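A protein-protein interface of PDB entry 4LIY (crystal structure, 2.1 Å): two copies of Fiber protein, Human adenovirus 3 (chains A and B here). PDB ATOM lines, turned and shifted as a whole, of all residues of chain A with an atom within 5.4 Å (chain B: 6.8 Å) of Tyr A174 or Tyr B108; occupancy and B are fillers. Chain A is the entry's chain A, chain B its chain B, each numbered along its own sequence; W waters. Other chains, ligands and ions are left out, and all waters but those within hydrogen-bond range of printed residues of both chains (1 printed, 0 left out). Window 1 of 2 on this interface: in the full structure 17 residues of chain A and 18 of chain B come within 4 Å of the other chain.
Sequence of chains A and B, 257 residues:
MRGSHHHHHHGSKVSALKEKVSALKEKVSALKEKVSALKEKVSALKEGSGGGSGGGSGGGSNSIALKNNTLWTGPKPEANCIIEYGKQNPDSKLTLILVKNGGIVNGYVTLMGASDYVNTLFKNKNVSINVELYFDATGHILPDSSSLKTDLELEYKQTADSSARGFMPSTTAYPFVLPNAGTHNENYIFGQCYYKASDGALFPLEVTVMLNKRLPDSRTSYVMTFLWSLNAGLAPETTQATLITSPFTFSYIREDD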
ATOM      1  N   ILE A 104      17.631 -10.369  -0.259  1.00  0.00           N
ATOM      2  CA  ILE A 104      18.371 -10.799   0.911  1.00  0.00           C
ATOM      3  C   ILE A 104      19.723 -10.121   1.011  1.00  0.00           C
ATOM      4  O   ILE A 104      20.206  -9.521   0.051  1.00  0.00           O
ATOM      5  CB  ILE A 104      18.583 -12.346   0.964  1.00  0.00           C
ATOM      6  CG1 ILE A 104      19.543 -12.808  -0.118  1.00  0.00           C
ATOM      7  CG2 ILE A 104      17.248 -13.088   0.856  1.00  0.00           C
ATOM      8  CD1 ILE A 104      20.060 -14.201   0.110  1.00  0.00           C
ATOM      9  N   PRO A 169      18.152  -5.954   8.716  1.00  0.00           N
ATOM     10  CA  PRO A 169      17.212  -7.082   8.752  1.00  0.00           C
ATOM     11  C   PRO A 169      15.766  -6.593   8.772  1.00  0.00           C
ATOM     12  O   PRO A 169      15.419  -5.692   9.546  1.00  0.00           O
ATOM     13  CB  PRO A 169      17.575  -7.807  10.046  1.00  0.00           C
ATOM     14  CG  PRO A 169      18.269  -6.750  10.903  1.00  0.00           C
ATOM     15  CD  PRO A 169      18.959  -5.846   9.946  1.00  0.00           C
ATOM     16  N   SER A 170      14.930  -7.176   7.924  1.00  0.00           N
ATOM     17  CA  SER A 170      13.523  -6.779   7.808  1.00  0.00           C
ATOM     18  C   SER A 170      12.809  -6.835   9.168  1.00  0.00           C
ATOM     19  O   SER A 170      12.902  -7.849   9.877  1.00  0.00           O
ATOM     20  CB  SER A 170      12.812  -7.730   6.847  1.00  0.00           C
ATOM     21  OG  SER A 170      11.416  -7.601   6.970  1.00  0.00           O
ATOM     22  N   THR A 171      12.056  -5.800   9.508  1.00  0.00           N
ATOM     23  CA  THR A 171      11.261  -5.823  10.751  1.00  0.00           C
ATOM     24  C   THR A 171       9.943  -6.539  10.481  1.00  0.00           C
ATOM     25  O   THR A 171       9.163  -6.781  11.402  1.00  0.00           O
ATOM     26  CB  THR A 171      10.949  -4.420  11.271  1.00  0.00           C
ATOM     27  OG1 THR A 171      10.437  -3.628  10.202  1.00  0.00           O
ATOM     28  CG2 THR A 171      12.194  -3.767  11.811  1.00  0.00           C
ATOM     29  N   THR A 172       9.698  -6.871   9.211  1.00  0.00           N
ATOM     30  CA  THR A 172       8.533  -7.667   8.850  1.00  0.00           C
ATOM     31  C   THR A 172       8.865  -9.144   8.976  1.00  0.00           C
ATOM     32  O   THR A 172       8.078  -9.900   9.522  1.00  0.00           O
ATOM     33  CB  THR A 172       8.072  -7.373   7.420  1.00  0.00           C
ATOM     34  OG1 THR A 172       7.641  -6.011   7.344  1.00  0.00           O
ATOM     35  CG2 THR A 172       6.904  -8.291   7.016  1.00  0.00           C
ATOM     36  N   ALA A 173      10.026  -9.557   8.463  1.00  0.00           N
ATOM     37  CA  ALA A 173      10.471 -10.936   8.631  1.00  0.00           C
ATOM     38  C   ALA A 173      10.924 -11.223  10.079  1.00  0.00           C
ATOM     39  O   ALA A 173      10.666 -12.306  10.610  1.00  0.00           O
ATOM     40  CB  ALA A 173      11.599 -11.250   7.657  1.00  0.00           C
ATOM     41  N   TYR A 174      11.624 -10.257  10.687  1.00  0.00           N
ATOM     42  CA  TYR A 174      12.209 -10.423  12.017  1.00  0.00           C
ATOM     43  C   TYR A 174      11.692  -9.285  12.881  1.00  0.00           C
ATOM     44  O   TYR A 174      12.339  -8.233  13.015  1.00  0.00           O
ATOM     45  CB  TYR A 174      13.732 -10.419  11.943  1.00  0.00           C
ATOM     46  CG  TYR A 174      14.245 -11.215  10.754  1.00  0.00           C
ATOM     47  CD1 TYR A 174      14.194 -12.610  10.746  1.00  0.00           C
ATOM     48  CD2 TYR A 174      14.754 -10.575   9.638  1.00  0.00           C
ATOM     49  CE1 TYR A 174      14.656 -13.342   9.652  1.00  0.00           C
ATOM     50  CE2 TYR A 174      15.234 -11.300   8.553  1.00  0.00           C
ATOM     51  CZ  TYR A 174      15.172 -12.682   8.570  1.00  0.00           C
ATOM     52  OH  TYR A 174      15.625 -13.408   7.505  1.00  0.00           O
ATOM     53  N   PRO A 175      10.488  -9.470  13.418  1.00  0.00           N
ATOM     54  CA  PRO A 175       9.806  -8.385  14.124  1.00  0.00           C
ATOM     55  C   PRO A 175      10.404  -8.102  15.504  1.00  0.00           C
ATOM     56  O   PRO A 175      11.092  -8.953  16.076  1.00  0.00           O
ATOM     57  CB  PRO A 175       8.375  -8.909  14.270  1.00  0.00           C
ATOM     58  CG  PRO A 175       8.532 -10.413  14.305  1.00  0.00           C
ATOM     59  CD  PRO A 175       9.680 -10.707  13.364  1.00  0.00           C
ATOM     60  N   PHE A 176      10.161  -6.896  15.993  1.00  0.00           N
ATOM     61  CA  PHE A 176      10.369  -6.567  17.404  1.00  0.00           C
ATOM     62  C   PHE A 176       9.153  -7.025  18.143  1.00  0.00           C
ATOM     63  O   PHE A 176       8.056  -6.902  17.626  1.00  0.00           O
ATOM     64  CB  PHE A 176      10.591  -5.074  17.567  1.00  0.00           C
ATOM     65  CG  PHE A 176      11.950  -4.651  17.133  1.00  0.00           C
ATOM     66  CD1 PHE A 176      13.049  -4.934  17.930  1.00  0.00           C
ATOM     67  CD2 PHE A 176      12.149  -4.046  15.896  1.00  0.00           C
ATOM     68  CE1 PHE A 176      14.309  -4.582  17.533  1.00  0.00           C
ATOM     69  CE2 PHE A 176      13.403  -3.684  15.490  1.00  0.00           C
ATOM     70  CZ  PHE A 176      14.496  -3.956  16.295  1.00  0.00           C
ATOM     71  N   GLU A 186      11.566 -17.208  15.231  1.00  0.00           N
ATOM     72  CA  GLU A 186      11.561 -16.554  13.922  1.00  0.00           C
ATOM     73  C   GLU A 186      12.673 -15.502  13.824  1.00  0.00           C
ATOM     74  O   GLU A 186      13.077 -15.149  12.741  1.00  0.00           O
ATOM     75  CB  GLU A 186      10.184 -15.955  13.566  1.00  0.00           C
ATOM     76  CG  GLU A 186       9.538 -15.169  14.670  1.00  0.00           C
ATOM     77  CD  GLU A 186       8.496 -15.978  15.422  1.00  0.00           C
ATOM     78  OE1 GLU A 186       8.849 -16.564  16.475  1.00  0.00           O
ATOM     79  OE2 GLU A 186       7.333 -16.029  14.956  1.00  0.00           O
ATOM     80  N   ASN A 187      13.186 -15.040  14.959  1.00  0.00           N
ATOM     81  CA  ASN A 187      14.215 -14.009  14.973  1.00  0.00           C
ATOM     82  C   ASN A 187      15.639 -14.560  15.012  1.00  0.00           C
ATOM     83  O   ASN A 187      16.605 -13.785  15.107  1.00  0.00           O
ATOM     84  CB  ASN A 187      14.013 -13.087  16.185  1.00  0.00           C
ATOM     85  CG  ASN A 187      12.746 -12.286  16.084  1.00  0.00           C
ATOM     86  OD1 ASN A 187      11.690 -12.748  16.511  1.00  0.00           O
ATOM     87  ND2 ASN A 187      12.829 -11.086  15.502  1.00  0.00           N
ATOM     88  N   ILE A 189      18.868 -17.129  13.588  1.00  0.00           N
ATOM     89  CA  ILE A 189      19.570 -17.982  12.659  1.00  0.00           C
ATOM     90  C   ILE A 189      20.611 -18.781  13.439  1.00  0.00           C
ATOM     91  O   ILE A 189      21.399 -18.202  14.184  1.00  0.00           O
ATOM     92  CB  ILE A 189      20.300 -17.121  11.608  1.00  0.00           C
ATOM     93  CG1 ILE A 189      19.289 -16.421  10.710  1.00  0.00           C
ATOM     94  CG2 ILE A 189      21.243 -17.968  10.780  1.00  0.00           C
ATOM     95  CD1 ILE A 189      19.911 -15.356   9.832  1.00  0.00           C
ATOM     96  N   LEU A 211      18.148 -11.366  15.157  1.00  0.00           N
ATOM     97  CA  LEU A 211      17.805 -10.211  14.354  1.00  0.00           C
ATOM     98  C   LEU A 211      16.616  -9.501  14.977  1.00  0.00           C
ATOM     99  O   LEU A 211      15.566 -10.105  15.212  1.00  0.00           O
ATOM    100  CB  LEU A 211      17.482 -10.636  12.930  1.00  0.00           C
ATOM    101  CG  LEU A 211      18.643 -11.339  12.228  1.00  0.00           C
ATOM    102  CD1 LEU A 211      18.232 -11.795  10.866  1.00  0.00           C
ATOM    103  CD2 LEU A 211      19.859 -10.426  12.133  1.00  0.00           C
ATOM    104  N   ASN A 212      16.793  -8.209  15.208  1.00  0.00           N
ATOM    105  CA  ASN A 212      15.768  -7.385  15.808  1.00  0.00           C
ATOM    106  C   ASN A 212      15.269  -8.029  17.125  1.00  0.00           C
ATOM    107  O   ASN A 212      16.073  -8.231  18.028  1.00  0.00           O
ATOM    108  CB  ASN A 212      14.678  -7.118  14.775  1.00  0.00           C
ATOM    109  CG  ASN A 212      15.206  -6.356  13.558  1.00  0.00           C
ATOM    110  OD1 ASN A 212      16.142  -5.546  13.668  1.00  0.00           O
ATOM    111  ND2 ASN A 212      14.615  -6.618  12.384  1.00  0.00           N
ATOM    112  N   LYS A 213      13.976  -8.349  17.215  1.00  0.00           N
ATOM    113  CA  LYS A 213      13.365  -9.026  18.368  1.00  0.00           C
ATOM    114  C   LYS A 213      13.236  -8.110  19.601  1.00  0.00           C
ATOM    115  O   LYS A 213      12.139  -7.845  20.067  1.00  0.00           O
ATOM    116  CB  LYS A 213      14.092 -10.317  18.779  1.00  0.00           C
ATOM    117  CG  LYS A 213      13.202 -11.236  19.645  1.00  0.00           C
ATOM    118  CD  LYS A 213      13.990 -12.179  20.543  1.00  0.00           C
ATOM    119  CE  LYS A 213      14.523 -11.471  21.791  1.00  0.00           C
ATOM    120  NZ  LYS A 213      15.280 -12.404  22.681  1.00  0.00           N
ATOM    121  N   SER A 251      22.447 -15.631   5.692  1.00  0.00           N
ATOM    122  CA  SER A 251      21.641 -14.784   4.835  1.00  0.00           C
ATOM    123  C   SER A 251      20.379 -14.437   5.559  1.00  0.00           C
ATOM    124  O   SER A 251      19.819 -15.265   6.264  1.00  0.00           O
ATOM    125  CB  SER A 251      21.253 -15.541   3.560  1.00  0.00           C
ATOM    126  OG  SER A 251      22.398 -15.754   2.793  1.00  0.00           O
ATOM    127  N   TYR A 252      19.903 -13.221   5.350  1.00  0.00           N
ATOM    128  CA  TYR A 252      18.659 -12.818   5.936  1.00  0.00           C
ATOM    129  C   TYR A 252      17.900 -11.912   5.001  1.00  0.00           C
ATOM    130  O   TYR A 252      18.480 -11.291   4.108  1.00  0.00           O
ATOM    131  CB  TYR A 252      18.892 -12.128   7.287  1.00  0.00           C
ATOM    132  CG  TYR A 252      19.757 -10.870   7.244  1.00  0.00           C
ATOM    133  CD1 TYR A 252      19.207  -9.623   6.964  1.00  0.00           C
ATOM    134  CD2 TYR A 252      21.109 -10.921   7.554  1.00  0.00           C
ATOM    135  CE1 TYR A 252      19.993  -8.459   6.973  1.00  0.00           C
ATOM    136  CE2 TYR A 252      21.906  -9.769   7.545  1.00  0.00           C
ATOM    137  CZ  TYR A 252      21.337  -8.547   7.252  1.00  0.00           C
ATOM    138  OH  TYR A 252      22.124  -7.413   7.242  1.00  0.00           O
ATOM    139  N   ILE A 253      16.588 -11.866   5.216  1.00  0.00           N
ATOM    140  CA  ILE A 253      15.692 -10.992   4.475  1.00  0.00           C
ATOM    141  C   ILE A 253      15.951  -9.543   4.879  1.00  0.00           C
ATOM    142  O   ILE A 253      15.923  -9.195   6.068  1.00  0.00           O
ATOM    143  CB  ILE A 253      14.239 -11.374   4.759  1.00  0.00           C
ATOM    144  CG1 ILE A 253      13.992 -12.832   4.371  1.00  0.00           C
ATOM    145  CG2 ILE A 253      13.273 -10.452   4.024  1.00  0.00           C
ATOM    146  CD1 ILE A 253      12.718 -13.426   4.934  1.00  0.00           C
ATOM    147  N   PRO B  75       8.257 -12.234   2.349  1.00  0.00           N
ATOM    148  CA  PRO B  75       8.997 -12.296   3.622  1.00  0.00           C
ATOM    149  C   PRO B  75       8.232 -12.864   4.808  1.00  0.00           C
ATOM    150  O   PRO B  75       8.870 -13.275   5.771  1.00  0.00           O
ATOM    151  CB  PRO B  75       9.342 -10.829   3.896  1.00  0.00           C
ATOM    152  CG  PRO B  75       8.255 -10.046   3.197  1.00  0.00           C
ATOM    153  CD  PRO B  75       7.855 -10.862   1.991  1.00  0.00           C
ATOM    154  N   LYS B  76       6.909 -12.885   4.763  1.00  0.00           N
ATOM    155  CA  LYS B  76       6.132 -13.327   5.916  1.00  0.00           C
ATOM    156  C   LYS B  76       4.796 -13.835   5.403  1.00  0.00           C
ATOM    157  O   LYS B  76       3.762 -13.237   5.618  1.00  0.00           O
ATOM    158  CB  LYS B  76       5.982 -12.175   6.933  1.00  0.00           C
ATOM    159  CG  LYS B  76       5.288 -12.527   8.252  1.00  0.00           C
ATOM    160  CD  LYS B  76       6.085 -13.523   9.067  1.00  0.00           C
ATOM    161  CE  LYS B  76       7.433 -12.973   9.475  1.00  0.00           C
ATOM    162  NZ  LYS B  76       8.054 -13.697  10.627  1.00  0.00           N
ATOM    163  N   THR B  95       8.409 -20.171   3.777  1.00  0.00           N
ATOM    164  CA  THR B  95       9.120 -19.006   3.250  1.00  0.00           C
ATOM    165  C   THR B  95      10.233 -19.572   2.360  1.00  0.00           C
ATOM    166  O   THR B  95      11.091 -20.327   2.827  1.00  0.00           O
ATOM    167  CB  THR B  95       9.734 -18.135   4.356  1.00  0.00           C
ATOM    168  OG1 THR B  95       8.720 -17.717   5.288  1.00  0.00           O
ATOM    169  CG2 THR B  95      10.399 -16.895   3.750  1.00  0.00           C
ATOM    170  N   LEU B  96      10.180 -19.266   1.068  1.00  0.00           N
ATOM    171  CA  LEU B  96      11.199 -19.741   0.126  1.00  0.00           C
ATOM    172  C   LEU B  96      11.633 -18.574  -0.715  1.00  0.00           C
ATOM    173  O   LEU B  96      10.793 -17.900  -1.333  1.00  0.00           O
ATOM    174  CB  LEU B  96      10.658 -20.864  -0.743  1.00  0.00           C
ATOM    175  CG  LEU B  96      11.624 -21.379  -1.820  1.00  0.00           C
ATOM    176  CD1 LEU B  96      12.851 -22.044  -1.216  1.00  0.00           C
ATOM    177  CD2 LEU B  96      10.907 -22.351  -2.676  1.00  0.00           C
ATOM    178  N   ILE B  97      12.941 -18.325  -0.737  1.00  0.00           N
ATOM    179  CA  ILE B  97      13.503 -17.180  -1.436  1.00  0.00           C
ATOM    180  C   ILE B  97      14.639 -17.657  -2.329  1.00  0.00           C
ATOM    181  O   ILE B  97      15.559 -18.332  -1.871  1.00  0.00           O
ATOM    182  CB  ILE B  97      14.018 -16.139  -0.444  1.00  0.00           C
ATOM    183  CG1 ILE B  97      12.898 -15.773   0.543  1.00  0.00           C
ATOM    184  CG2 ILE B  97      14.519 -14.889  -1.171  1.00  0.00           C
ATOM    185  CD1 ILE B  97      13.300 -14.733   1.547  1.00  0.00           C
ATOM    186  N   LEU B  98      14.537 -17.363  -3.616  1.00  0.00           N
ATOM    187  CA  LEU B  98      15.510 -17.830  -4.593  1.00  0.00           C
ATOM    188  C   LEU B  98      16.067 -16.606  -5.296  1.00  0.00           C
ATOM    189  O   LEU B  98      15.328 -15.881  -5.977  1.00  0.00           O
ATOM    190  CB  LEU B  98      14.852 -18.769  -5.602  1.00  0.00           C
ATOM    191  CG  LEU B  98      14.145 -20.010  -5.054  1.00  0.00           C
ATOM    192  CD1 LEU B  98      13.463 -20.722  -6.191  1.00  0.00           C
ATOM    193  CD2 LEU B  98      15.108 -20.948  -4.358  1.00  0.00           C
ATOM    194  N   VAL B  99      17.353 -16.344  -5.097  1.00  0.00           N
ATOM    195  CA  VAL B  99      17.988 -15.171  -5.706  1.00  0.00           C
ATOM    196  C   VAL B  99      18.994 -15.578  -6.772  1.00  0.00           C
ATOM    197  O   VAL B  99      19.937 -16.333  -6.513  1.00  0.00           O
ATOM    198  CB  VAL B  99      18.721 -14.315  -4.673  1.00  0.00           C
ATOM    199  CG1 VAL B  99      19.341 -13.094  -5.344  1.00  0.00           C
ATOM    200  CG2 VAL B  99      17.761 -13.901  -3.554  1.00  0.00           C
ATOM    201  N   ASN B 106      21.027 -18.529  -5.091  1.00  0.00           N
ATOM    202  CA  ASN B 106      21.167 -18.625  -3.623  1.00  0.00           C
ATOM    203  C   ASN B 106      19.781 -18.745  -3.021  1.00  0.00           C
ATOM    204  O   ASN B 106      18.907 -17.910  -3.290  1.00  0.00           O
ATOM    205  CB  ASN B 106      21.846 -17.381  -3.046  1.00  0.00           C
ATOM    206  CG  ASN B 106      23.267 -17.182  -3.580  1.00  0.00           C
ATOM    207  OD1 ASN B 106      23.606 -16.107  -4.073  1.00  0.00           O
ATOM    208  ND2 ASN B 106      24.096 -18.211  -3.481  1.00  0.00           N
ATOM    209  N   GLY B 107      19.561 -19.790  -2.243  1.00  0.00           N
ATOM    210  CA  GLY B 107      18.251 -20.071  -1.711  1.00  0.00           C
ATOM    211  C   GLY B 107      18.224 -19.881  -0.195  1.00  0.00           C
ATOM    212  O   GLY B 107      19.240 -20.012   0.483  1.00  0.00           O
ATOM    213  N   TYR B 108      17.042 -19.598   0.329  1.00  0.00           N
ATOM    214  CA  TYR B 108      16.835 -19.393   1.757  1.00  0.00           C
ATOM    215  C   TYR B 108      15.473 -20.005   1.992  1.00  0.00           C
ATOM    216  O   TYR B 108      14.518 -19.651   1.305  1.00  0.00           O
ATOM    217  CB  TYR B 108      16.872 -17.896   2.063  1.00  0.00           C
ATOM    218  CG  TYR B 108      16.375 -17.412   3.436  1.00  0.00           C
ATOM    219  CD1 TYR B 108      15.020 -17.464   3.781  1.00  0.00           C
ATOM    220  CD2 TYR B 108      17.248 -16.828   4.347  1.00  0.00           C
ATOM    221  CE1 TYR B 108      14.555 -16.973   5.029  1.00  0.00           C
ATOM    222  CE2 TYR B 108      16.793 -16.337   5.607  1.00  0.00           C
ATOM    223  CZ  TYR B 108      15.438 -16.406   5.930  1.00  0.00           C
ATOM    224  OH  TYR B 108      14.963 -15.924   7.160  1.00  0.00           O
ATOM    225  N   VAL B 109      15.381 -20.958   2.916  1.00  0.00           N
ATOM    226  CA  VAL B 109      14.104 -21.602   3.178  1.00  0.00           C
ATOM    227  C   VAL B 109      13.873 -21.787   4.700  1.00  0.00           C
ATOM    228  O   VAL B 109      14.786 -22.167   5.446  1.00  0.00           O
ATOM    229  CB  VAL B 109      14.002 -22.943   2.409  1.00  0.00           C
ATOM    230  CG1 VAL B 109      15.025 -23.931   2.926  1.00  0.00           C
ATOM    231  CG2 VAL B 109      12.615 -23.530   2.499  1.00  0.00           C
ATOM    232  N   THR B 110      12.658 -21.491   5.148  1.00  0.00           N
ATOM    233  CA  THR B 110      12.237 -21.808   6.520  1.00  0.00           C
ATOM    234  C   THR B 110      10.757 -22.193   6.487  1.00  0.00           C
ATOM    235  O   THR B 110       9.985 -21.684   5.675  1.00  0.00           O
ATOM    236  CB  THR B 110      12.513 -20.647   7.530  1.00  0.00           C
ATOM    237  OG1 THR B 110      11.882 -20.919   8.788  1.00  0.00           O
ATOM    238  CG2 THR B 110      11.982 -19.340   7.029  1.00  0.00           C
ATOM    239  N   PHE B 226      12.342 -30.730  -0.390  1.00  0.00           N
ATOM    240  CA  PHE B 226      13.025 -30.529   0.886  1.00  0.00           C
ATOM    241  C   PHE B 226      12.588 -31.610   1.849  1.00  0.00           C
ATOM    242  O   PHE B 226      11.416 -32.001   1.879  1.00  0.00           O
ATOM    243  CB  PHE B 226      12.694 -29.172   1.479  1.00  0.00           C
ATOM    244  CG  PHE B 226      13.072 -28.021   0.591  1.00  0.00           C
ATOM    245  CD1 PHE B 226      14.338 -27.481   0.651  1.00  0.00           C
ATOM    246  CD2 PHE B 226      12.153 -27.482  -0.307  1.00  0.00           C
ATOM    247  CE1 PHE B 226      14.686 -26.417  -0.156  1.00  0.00           C
ATOM    248  CE2 PHE B 226      12.499 -26.420  -1.130  1.00  0.00           C
ATOM    249  CZ  PHE B 226      13.766 -25.889  -1.054  1.00  0.00           C
ATOM    250  N   PRO B 247      16.450 -20.844   9.527  1.00  0.00           N
ATOM    251  CA  PRO B 247      16.739 -20.670   8.104  1.00  0.00           C
ATOM    252  C   PRO B 247      17.849 -21.576   7.551  1.00  0.00           C
ATOM    253  O   PRO B 247      18.925 -21.713   8.135  1.00  0.00           O
ATOM    254  CB  PRO B 247      17.151 -19.204   8.012  1.00  0.00           C
ATOM    255  CG  PRO B 247      16.379 -18.520   9.146  1.00  0.00           C
ATOM    256  CD  PRO B 247      16.323 -19.558  10.243  1.00  0.00           C
ATOM    257  N   PHE B 248      17.562 -22.181   6.405  1.00  0.00           N
ATOM    258  CA  PHE B 248      18.517 -23.033   5.703  1.00  0.00           C
ATOM    259  C   PHE B 248      18.847 -22.353   4.387  1.00  0.00           C
ATOM    260  O   PHE B 248      17.941 -21.949   3.644  1.00  0.00           O
ATOM    261  CB  PHE B 248      17.934 -24.435   5.469  1.00  0.00           C
ATOM    262  CG  PHE B 248      18.825 -25.327   4.653  1.00  0.00           C
ATOM    263  CD1 PHE B 248      19.980 -25.852   5.204  1.00  0.00           C
ATOM    264  CD2 PHE B 248      18.520 -25.626   3.336  1.00  0.00           C
ATOM    265  CE1 PHE B 248      20.817 -26.674   4.459  1.00  0.00           C
ATOM    266  CE2 PHE B 248      19.365 -26.435   2.584  1.00  0.00           C
ATOM    267  CZ  PHE B 248      20.513 -26.956   3.146  1.00  0.00           C
ATOM    268  N   THR B 249      20.137 -22.174   4.130  1.00  0.00           N
ATOM    269  CA  THR B 249      20.594 -21.520   2.914  1.00  0.00           C
ATOM    270  C   THR B 249      21.288 -22.561   2.039  1.00  0.00           C
ATOM    271  O   THR B 249      21.888 -23.511   2.532  1.00  0.00           O
ATOM    272  CB  THR B 249      21.584 -20.384   3.232  1.00  0.00           C
ATOM    273  OG1 THR B 249      22.650 -20.924   4.011  1.00  0.00           O
ATOM    274  CG2 THR B 249      20.897 -19.288   4.031  1.00  0.00           C
ATOM    275  N   PHE B 250      21.204 -22.398   0.733  1.00  0.00           N
ATOM    276  CA  PHE B 250      21.827 -23.352  -0.165  1.00  0.00           C
ATOM    277  C   PHE B 250      21.987 -22.651  -1.486  1.00  0.00           C
ATOM    278  O   PHE B 250      21.406 -21.563  -1.684  1.00  0.00           O
ATOM    279  CB  PHE B 250      20.963 -24.614  -0.301  1.00  0.00           C
ATOM    280  CG  PHE B 250      19.551 -24.343  -0.762  1.00  0.00           C
ATOM    281  CD1 PHE B 250      18.602 -23.838   0.120  1.00  0.00           C
ATOM    282  CD2 PHE B 250      19.174 -24.576  -2.073  1.00  0.00           C
ATOM    283  CE1 PHE B 250      17.299 -23.573  -0.302  1.00  0.00           C
ATOM    284  CE2 PHE B 250      17.868 -24.308  -2.499  1.00  0.00           C
ATOM    285  CZ  PHE B 250      16.941 -23.794  -1.613  1.00  0.00           C
HETATM  286  O   HOH W   1       6.765 -13.907  13.068  1.00  0.00           O
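The side-chain hydroxyl (OH) of Tyr A174 sits at hydrogen-bond distance from the side-chain hydroxyl (OH) of Tyr B108.
The side-chain amino group of Lys B76 sits at hydrogen-bond distance from the backbone carbonyl oxygen of Ala A173 (3.0 Å).
The backbone NH of Ala A173 sits at hydrogen-bond distance from the side-chain hydroxyl of Ser A170 (2.8 Å).
The backbone carbonyl oxygen (O) of Tyr A174 is in hydrogen-bond range of the side-chain amide nitrogen (ND2) of Asn A212, 2.9 Å away.
The backbone NH (N) of Ile A253 sits at hydrogen-bond distance from the side-chain hydroxyl (OH) of Tyr A174, at 2.9 Å.
N of Ile B97 lies within hydrogen-bond range of O of Tyr B108.
The backbone NH of Ser A170 sits at hydrogen-bond distance from the backbone carbonyl oxygen of Ile A253 (2.9 Å).
OG of Ser A170 lies within hydrogen-bond range of N of Thr A172 (2.9 Å).
Among the printed residues, pairs that only touch across the chains: Ile A104 with Ile B97, Thr A172 with Lys B76, Ala A173 with Pro B75, Ile A189 with Pro B247, Ser A251 with Tyr B108, Ser A251 with Thr B249, Tyr A252 with Tyr B108, Ile A253 with Pro B75, Ile A253 with Ile B97 and Ile A253 with Tyr B108.
Of the printed residues of chain B, Ile A104 touches Ile B97.
Of the printed residues of chain B, Ala A173 touches Pro B75 and Lys B76.
Of chain B, only Tyr B108 comes within 4 Å of Tyr A174.
Glu A186 touches none of the printed residues of chain B.
Of the printed residues of chain B, Ile A189 touches Pro B247.
Printed residues of chain A within 4 Å of Lys B76: Thr A172 (3.1 Å) and Ala A173 (3.0 Å).
Phe B226 touches none of the printed residues of chain A.
The nearest residue of chain B that does not touch Tyr A174 is Lys B76 (5.0 Å).
The nearest printed residue of chain B that does not touch Ala A173 is Tyr B108 (5.8 Å).
Along chain A the printed residues that touch a printed residue of chain B span positions 104 to 253.
Printed residues of chain B that touch a printed residue of chain A: Pro B75, Lys B76, Ile B97, Tyr B108, Pro B247 and Thr B249.
Hydrophobic or aromatic side chains of chain B that line the printed part of chain A: Pro B75, Ile B97, Tyr B108 and Pro B247.
No position is printed for both chains.
Of the 12 pairs that touch across the chains among the printed residues, none has its exchanged pair printed and touching as well.
Water W1 bridges NZ of Lys B76 (2.8 Å) and OE2 of Glu A186 (2.9 Å).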
